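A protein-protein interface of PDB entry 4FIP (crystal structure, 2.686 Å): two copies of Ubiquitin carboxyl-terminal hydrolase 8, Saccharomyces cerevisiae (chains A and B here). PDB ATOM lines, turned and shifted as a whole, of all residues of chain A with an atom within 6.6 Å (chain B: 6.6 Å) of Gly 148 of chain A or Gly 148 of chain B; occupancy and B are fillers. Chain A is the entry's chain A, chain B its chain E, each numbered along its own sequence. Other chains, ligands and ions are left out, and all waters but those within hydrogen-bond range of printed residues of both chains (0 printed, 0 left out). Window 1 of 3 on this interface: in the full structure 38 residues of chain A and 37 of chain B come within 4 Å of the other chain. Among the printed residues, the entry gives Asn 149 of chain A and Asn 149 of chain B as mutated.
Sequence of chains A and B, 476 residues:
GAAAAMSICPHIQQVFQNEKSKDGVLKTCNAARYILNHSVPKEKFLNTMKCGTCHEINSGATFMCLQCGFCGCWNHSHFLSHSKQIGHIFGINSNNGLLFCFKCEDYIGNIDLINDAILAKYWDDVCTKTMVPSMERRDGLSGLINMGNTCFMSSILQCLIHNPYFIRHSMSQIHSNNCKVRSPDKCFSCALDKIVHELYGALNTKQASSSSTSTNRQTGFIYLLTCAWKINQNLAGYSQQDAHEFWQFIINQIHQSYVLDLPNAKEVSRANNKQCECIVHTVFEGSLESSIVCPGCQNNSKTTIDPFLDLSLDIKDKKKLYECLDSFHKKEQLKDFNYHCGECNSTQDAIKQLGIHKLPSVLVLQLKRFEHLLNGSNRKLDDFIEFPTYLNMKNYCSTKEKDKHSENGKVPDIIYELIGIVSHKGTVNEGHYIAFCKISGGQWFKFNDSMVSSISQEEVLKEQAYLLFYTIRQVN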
ATOM      1  N   ILE A 145     -19.622 -17.609 -16.338  1.00  0.00           N
ATOM      2  CA  ILE A 145     -20.816 -17.688 -15.524  1.00  0.00           C
ATOM      3  C   ILE A 145     -21.996 -18.159 -16.359  1.00  0.00           C
ATOM      4  O   ILE A 145     -22.472 -17.381 -17.212  1.00  0.00           O
ATOM      5  CB  ILE A 145     -21.207 -16.257 -15.065  1.00  0.00           C
ATOM      6  CG1 ILE A 145     -20.040 -15.532 -14.370  1.00  0.00           C
ATOM      7  CG2 ILE A 145     -22.446 -16.309 -14.177  1.00  0.00           C
ATOM      8  CD1 ILE A 145     -20.451 -14.193 -13.784  1.00  0.00           C
ATOM      9  N   ASN A 146     -22.497 -19.386 -16.146  1.00  0.00           N
ATOM     10  CA  ASN A 146     -23.695 -19.811 -16.900  1.00  0.00           C
ATOM     11  C   ASN A 146     -24.981 -19.271 -16.242  1.00  0.00           C
ATOM     12  O   ASN A 146     -24.897 -18.286 -15.508  1.00  0.00           O
ATOM     13  CB  ASN A 146     -23.673 -21.311 -17.324  1.00  0.00           C
ATOM     14  CG  ASN A 146     -24.074 -22.280 -16.240  1.00  0.00           C
ATOM     15  OD1 ASN A 146     -24.268 -21.911 -15.087  1.00  0.00           O
ATOM     16  ND2 ASN A 146     -24.198 -23.546 -16.618  1.00  0.00           N
ATOM     17  N   MET A 147     -26.158 -19.821 -16.552  1.00  0.00           N
ATOM     18  CA  MET A 147     -27.425 -19.365 -15.917  1.00  0.00           C
ATOM     19  C   MET A 147     -27.622 -20.036 -14.545  1.00  0.00           C
ATOM     20  O   MET A 147     -28.378 -19.550 -13.708  1.00  0.00           O
ATOM     21  CB  MET A 147     -28.634 -19.657 -16.830  1.00  0.00           C
ATOM     22  CG  MET A 147     -29.858 -18.768 -16.590  1.00  0.00           C
ATOM     23  SD  MET A 147     -30.194 -17.518 -17.864  1.00  0.00           S
ATOM     24  CE  MET A 147     -31.487 -16.627 -17.024  1.00  0.00           C
ATOM     25  N   GLY A 148     -26.901 -21.138 -14.320  1.00  0.00           N
ATOM     26  CA  GLY A 148     -27.119 -22.019 -13.176  1.00  0.00           C
ATOM     27  C   GLY A 148     -28.044 -23.113 -13.653  1.00  0.00           C
ATOM     28  O   GLY A 148     -28.446 -23.094 -14.820  1.00  0.00           O
ATOM     29  N   ASN A 149     -28.368 -24.062 -12.775  1.00  0.00           N
ATOM     30  CA  ASN A 149     -29.402 -25.060 -13.078  1.00  0.00           C
ATOM     31  C   ASN A 149     -30.758 -24.459 -12.863  1.00  0.00           C
ATOM     32  O   ASN A 149     -30.942 -23.654 -11.950  1.00  0.00           O
ATOM     33  CB  ASN A 149     -29.241 -26.319 -12.250  1.00  0.00           C
ATOM     34  CG  ASN A 149     -28.066 -27.133 -12.718  1.00  0.00           C
ATOM     35  OD1 ASN A 149     -28.139 -27.808 -13.750  1.00  0.00           O
ATOM     36  ND2 ASN A 149     -26.946 -27.022 -12.003  1.00  0.00           N
ATOM     37  N   THR A 150     -31.706 -24.845 -13.708  1.00  0.00           N
ATOM     38  CA  THR A 150     -32.958 -24.099 -13.810  1.00  0.00           C
ATOM     39  C   THR A 150     -34.212 -24.785 -13.224  1.00  0.00           C
ATOM     40  O   THR A 150     -35.306 -24.250 -13.367  1.00  0.00           O
ATOM     41  CB  THR A 150     -33.197 -23.657 -15.267  1.00  0.00           C
ATOM     42  OG1 THR A 150     -33.240 -24.808 -16.124  1.00  0.00           O
ATOM     43  CG2 THR A 150     -32.078 -22.734 -15.692  1.00  0.00           C
ATOM     44  N   PHE A 152     -35.252 -24.975 -10.133  1.00  0.00           N
ATOM     45  CA  PHE A 152     -35.953 -24.069  -9.227  1.00  0.00           C
ATOM     46  C   PHE A 152     -36.967 -23.153  -9.930  1.00  0.00           C
ATOM     47  O   PHE A 152     -37.739 -22.475  -9.258  1.00  0.00           O
ATOM     48  CB  PHE A 152     -34.941 -23.223  -8.420  1.00  0.00           C
ATOM     49  CG  PHE A 152     -34.397 -22.024  -9.156  1.00  0.00           C
ATOM     50  CD1 PHE A 152     -33.314 -22.145 -10.025  1.00  0.00           C
ATOM     51  CD2 PHE A 152     -34.948 -20.763  -8.964  1.00  0.00           C
ATOM     52  CE1 PHE A 152     -32.810 -21.047 -10.700  1.00  0.00           C
ATOM     53  CE2 PHE A 152     -34.435 -19.665  -9.641  1.00  0.00           C
ATOM     54  CZ  PHE A 152     -33.367 -19.816 -10.506  1.00  0.00           C
ATOM     55  N   MET A 153     -36.944 -23.100 -11.259  1.00  0.00           N
ATOM     56  CA  MET A 153     -37.946 -22.377 -12.020  1.00  0.00           C
ATOM     57  C   MET A 153     -38.933 -23.338 -12.644  1.00  0.00           C
ATOM     58  O   MET A 153     -40.146 -23.140 -12.497  1.00  0.00           O
ATOM     59  CB  MET A 153     -37.294 -21.548 -13.102  1.00  0.00           C
ATOM     60  CG  MET A 153     -36.462 -20.435 -12.525  1.00  0.00           C
ATOM     61  SD  MET A 153     -35.697 -19.401 -13.787  1.00  0.00           S
ATOM     62  CE  MET A 153     -34.342 -20.476 -14.270  1.00  0.00           C
ATOM     63  N   ASN A 234     -28.812 -12.230 -12.319  1.00  0.00           N
ATOM     64  CA  ASN A 234     -28.311 -13.081 -11.211  1.00  0.00           C
ATOM     65  C   ASN A 234     -27.808 -14.468 -11.658  1.00  0.00           C
ATOM     66  O   ASN A 234     -28.166 -14.983 -12.726  1.00  0.00           O
ATOM     67  CB  ASN A 234     -29.362 -13.229 -10.088  1.00  0.00           C
ATOM     68  CG  ASN A 234     -30.743 -13.544 -10.624  1.00  0.00           C
ATOM     69  OD1 ASN A 234     -30.957 -14.587 -11.262  1.00  0.00           O
ATOM     70  ND2 ASN A 234     -31.689 -12.642 -10.383  1.00  0.00           N
ATOM     71  N   ASN B 146     -33.671 -28.661 -18.395  1.00  0.00           N
ATOM     72  CA  ASN B 146     -32.755 -27.935 -17.529  1.00  0.00           C
ATOM     73  C   ASN B 146     -31.700 -27.311 -18.396  1.00  0.00           C
ATOM     74  O   ASN B 146     -31.140 -27.998 -19.237  1.00  0.00           O
ATOM     75  CB  ASN B 146     -32.119 -28.873 -16.498  1.00  0.00           C
ATOM     76  CG  ASN B 146     -31.469 -28.129 -15.342  1.00  0.00           C
ATOM     77  OD1 ASN B 146     -31.974 -28.124 -14.215  1.00  0.00           O
ATOM     78  ND2 ASN B 146     -30.349 -27.492 -15.615  1.00  0.00           N
ATOM     79  N   MET B 147     -31.432 -26.021 -18.172  1.00  0.00           N
ATOM     80  CA  MET B 147     -30.510 -25.206 -19.010  1.00  0.00           C
ATOM     81  C   MET B 147     -29.138 -24.904 -18.369  1.00  0.00           C
ATOM     82  O   MET B 147     -28.446 -23.964 -18.773  1.00  0.00           O
ATOM     83  CB  MET B 147     -31.154 -23.858 -19.346  1.00  0.00           C
ATOM     84  CG  MET B 147     -32.649 -23.883 -19.634  1.00  0.00           C
ATOM     85  SD  MET B 147     -33.063 -23.699 -21.367  1.00  0.00           S
ATOM     86  CE  MET B 147     -32.590 -25.336 -21.902  1.00  0.00           C
ATOM     87  N   GLY B 148     -28.760 -25.673 -17.356  1.00  0.00           N
ATOM     88  CA  GLY B 148     -27.420 -25.618 -16.803  1.00  0.00           C
ATOM     89  C   GLY B 148     -26.424 -26.464 -17.602  1.00  0.00           C
ATOM     90  O   GLY B 148     -25.276 -26.573 -17.204  1.00  0.00           O
ATOM     91  N   ASN B 149     -26.857 -27.075 -18.718  1.00  0.00           N
ATOM     92  CA  ASN B 149     -25.929 -27.731 -19.653  1.00  0.00           C
ATOM     93  C   ASN B 149     -25.200 -26.705 -20.532  1.00  0.00           C
ATOM     94  O   ASN B 149     -25.707 -26.288 -21.587  1.00  0.00           O
ATOM     95  CB  ASN B 149     -26.648 -28.751 -20.549  1.00  0.00           C
ATOM     96  CG  ASN B 149     -25.679 -29.528 -21.437  1.00  0.00           C
ATOM     97  OD1 ASN B 149     -24.508 -29.642 -21.097  1.00  0.00           O
ATOM     98  ND2 ASN B 149     -26.156 -30.054 -22.570  1.00  0.00           N
ATOM     99  N   THR B 150     -23.991 -26.341 -20.108  1.00  0.00           N
ATOM    100  CA  THR B 150     -23.260 -25.205 -20.675  1.00  0.00           C
ATOM    101  C   THR B 150     -21.847 -25.511 -21.170  1.00  0.00           C
ATOM    102  O   THR B 150     -21.377 -24.852 -22.091  1.00  0.00           O
ATOM    103  CB  THR B 150     -23.199 -24.089 -19.623  1.00  0.00           C
ATOM    104  OG1 THR B 150     -24.254 -23.170 -19.893  1.00  0.00           O
ATOM    105  CG2 THR B 150     -21.854 -23.376 -19.612  1.00  0.00           C
ATOM    106  N   CYS B 151     -21.173 -26.500 -20.590  1.00  0.00           N
ATOM    107  CA  CYS B 151     -19.730 -26.597 -20.776  1.00  0.00           C
ATOM    108  C   CYS B 151     -19.283 -26.930 -22.214  1.00  0.00           C
ATOM    109  O   CYS B 151     -18.110 -26.816 -22.536  1.00  0.00           O
ATOM    110  CB  CYS B 151     -19.138 -27.589 -19.777  1.00  0.00           C
ATOM    111  SG  CYS B 151     -19.825 -29.250 -19.922  1.00  0.00           S
ATOM    112  N   TRP B 229     -29.927 -19.862 -27.714  1.00  0.00           N
ATOM    113  CA  TRP B 229     -31.107 -20.723 -27.517  1.00  0.00           C
ATOM    114  C   TRP B 229     -32.294 -20.274 -28.306  1.00  0.00           C
ATOM    115  O   TRP B 229     -33.082 -21.091 -28.733  1.00  0.00           O
ATOM    116  CB  TRP B 229     -31.530 -20.760 -26.057  1.00  0.00           C
ATOM    117  CG  TRP B 229     -30.549 -21.376 -25.098  1.00  0.00           C
ATOM    118  CD1 TRP B 229     -29.705 -22.465 -25.310  1.00  0.00           C
ATOM    119  CD2 TRP B 229     -30.308 -20.974 -23.706  1.00  0.00           C
ATOM    120  NE1 TRP B 229     -28.964 -22.739 -24.184  1.00  0.00           N
ATOM    121  CE2 TRP B 229     -29.283 -21.891 -23.187  1.00  0.00           C
ATOM    122  CE3 TRP B 229     -30.821 -19.983 -22.872  1.00  0.00           C
ATOM    123  CZ2 TRP B 229     -28.803 -21.794 -21.900  1.00  0.00           C
ATOM    124  CZ3 TRP B 229     -30.339 -19.894 -21.571  1.00  0.00           C
ATOM    125  CH2 TRP B 229     -29.347 -20.777 -21.096  1.00  0.00           C
ATOM    126  N   GLY B 237     -30.561 -27.528 -22.913  1.00  0.00           N
ATOM    127  CA  GLY B 237     -30.984 -28.720 -22.203  1.00  0.00           C
ATOM    128  C   GLY B 237     -29.841 -29.688 -22.110  1.00  0.00           C
ATOM    129  O   GLY B 237     -28.775 -29.438 -22.673  1.00  0.00           O
ATOM    130  N   TYR B 238     -30.059 -30.783 -21.385  1.00  0.00           N
ATOM    131  CA  TYR B 238     -29.113 -31.894 -21.352  1.00  0.00           C
ATOM    132  C   TYR B 238     -29.529 -32.910 -22.424  1.00  0.00           C
ATOM    133  O   TYR B 238     -30.049 -33.980 -22.120  1.00  0.00           O
ATOM    134  CB  TYR B 238     -29.055 -32.526 -19.956  1.00  0.00           C
ATOM    135  CG  TYR B 238     -28.439 -31.621 -18.895  1.00  0.00           C
ATOM    136  CD1 TYR B 238     -29.178 -30.568 -18.318  1.00  0.00           C
ATOM    137  CD2 TYR B 238     -27.121 -31.810 -18.459  1.00  0.00           C
ATOM    138  CE1 TYR B 238     -28.621 -29.738 -17.347  1.00  0.00           C
ATOM    139  CE2 TYR B 238     -26.558 -30.980 -17.488  1.00  0.00           C
ATOM    140  CZ  TYR B 238     -27.311 -29.949 -16.939  1.00  0.00           C
ATOM    141  OH  TYR B 238     -26.757 -29.131 -15.984  1.00  0.00           O
ATOM    142  N   ASP B 449     -15.843 -24.472 -16.161  1.00  0.00           N
ATOM    143  CA  ASP B 449     -16.754 -23.346 -15.819  1.00  0.00           C
ATOM    144  C   ASP B 449     -17.309 -23.407 -14.381  1.00  0.00           C
ATOM    145  O   ASP B 449     -18.006 -24.364 -14.047  1.00  0.00           O
ATOM    146  CB  ASP B 449     -17.898 -23.193 -16.868  1.00  0.00           C
ATOM    147  CG  ASP B 449     -19.034 -24.289 -16.765  1.00  0.00           C
ATOM    148  OD1 ASP B 449     -18.778 -25.458 -16.371  1.00  0.00           O
ATOM    149  OD2 ASP B 449     -20.205 -23.963 -17.123  1.00  0.00           O
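The side-chain hydroxyl (OG1) of Thr 150 of chain A sits at hydrogen-bond distance from the backbone NH (N) of Met 147 of chain B (3.0 Å). OH of Tyr 238 of chain B lies within hydrogen-bond range of OD1 of Asn 149 of chain A (2.9 Å). The side-chain amide nitrogen (ND2) of Asn 146 of chain B is in hydrogen-bond range of the side-chain amide oxygen (OD1) of Asn 149 of chain A. The side-chain amide nitrogen (ND2) of Asn 146 of chain A lies close to the side-chain hydroxyl (OG1) of Thr 150 of chain B. The side-chain amide nitrogen of Asn 146 of chain A is in hydrogen-bond range of the backbone carbonyl oxygen of Gly 148 of chain B, 3.3 Å away. The side-chain amide oxygen of Asn 146 of chain B lies within hydrogen-bond range of the backbone NH of Thr 150 of chain A (3.3 Å).
Asn 146 of chain A touches Gly 148 of chain B, but with the chains exchanged Gly 148 of chain A does not touch Asn 146 of chain B (4.9 Å). Asn 146 of chain A touches Thr 150 of chain B, and with the chains exchanged Thr 150 of chain A touches Asn 146 of chain B. Gly 148 of chain A touches its own counterpart, Gly 148 of chain B. Asn 149 of chain A touches Gly 148 of chain B, but with the chains exchanged Gly 148 of chain A does not touch Asn 149 of chain B (5.8 Å). Positions printed for both chains: 146, 147, 148, 149 and 150. Of the 8 pairs that touch across the chains among the printed residues, 3 have their exchanged pair printed and touching as well.
N of Asn 149 of chain B lies close to OH of Tyr 238 of chain B (3.4 Å). The backbone NH of Gly 148 of chain B sits close to the side-chain amide nitrogen of Asn 146 of chain B, 3.0 Å away. The side-chain hydroxyl (OH) of Tyr 238 of chain B sits close to the backbone carbonyl oxygen (O) of Gly 148 of chain B, at 3.2 Å. The backbone NH (N) of Gly 148 of chain A sits at hydrogen-bond distance from the side-chain amide oxygen (OD1) of Asn 146 of chain A.
Of the printed residues of chain B, Asn 146 of chain A touches Gly 148 (3.3 Å) and Thr 150 (3.2 Å). Of the printed residues of chain B, Asn 149 of chain A touches Asn 146 (2.9 Å), Gly 148 (3.8 Å) and Tyr 238 (2.9 Å). Of the printed residues of chain B, Thr 150 of chain A touches Asn 146 (3.3 Å) and Met 147 (3.0 Å). Of chain A, only Asn 146 (3.3 Å), Gly 148 (3.4 Å) and Asn 149 (3.8 Å) come within 4 Å of Gly 148 of chain B. The nearest residue of chain A that does not touch Gly 148 of chain B is Thr 150 of chain A (4.7 Å).
Of the 9 printed residues of chain A, 4 touch a printed residue of chain B. Along chain A the printed residues that touch a printed residue of chain B span positions 146 to 150. Printed residues of chain B that touch a printed residue of chain A: Asn 146, Met 147, Gly 148, Thr 150 and Tyr 238.
O of Gly 148 of chain A touches CA of Gly 148 of chain B, 3.4 Å away. Asn 149 of chain A touches Gly 148 of chain B.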
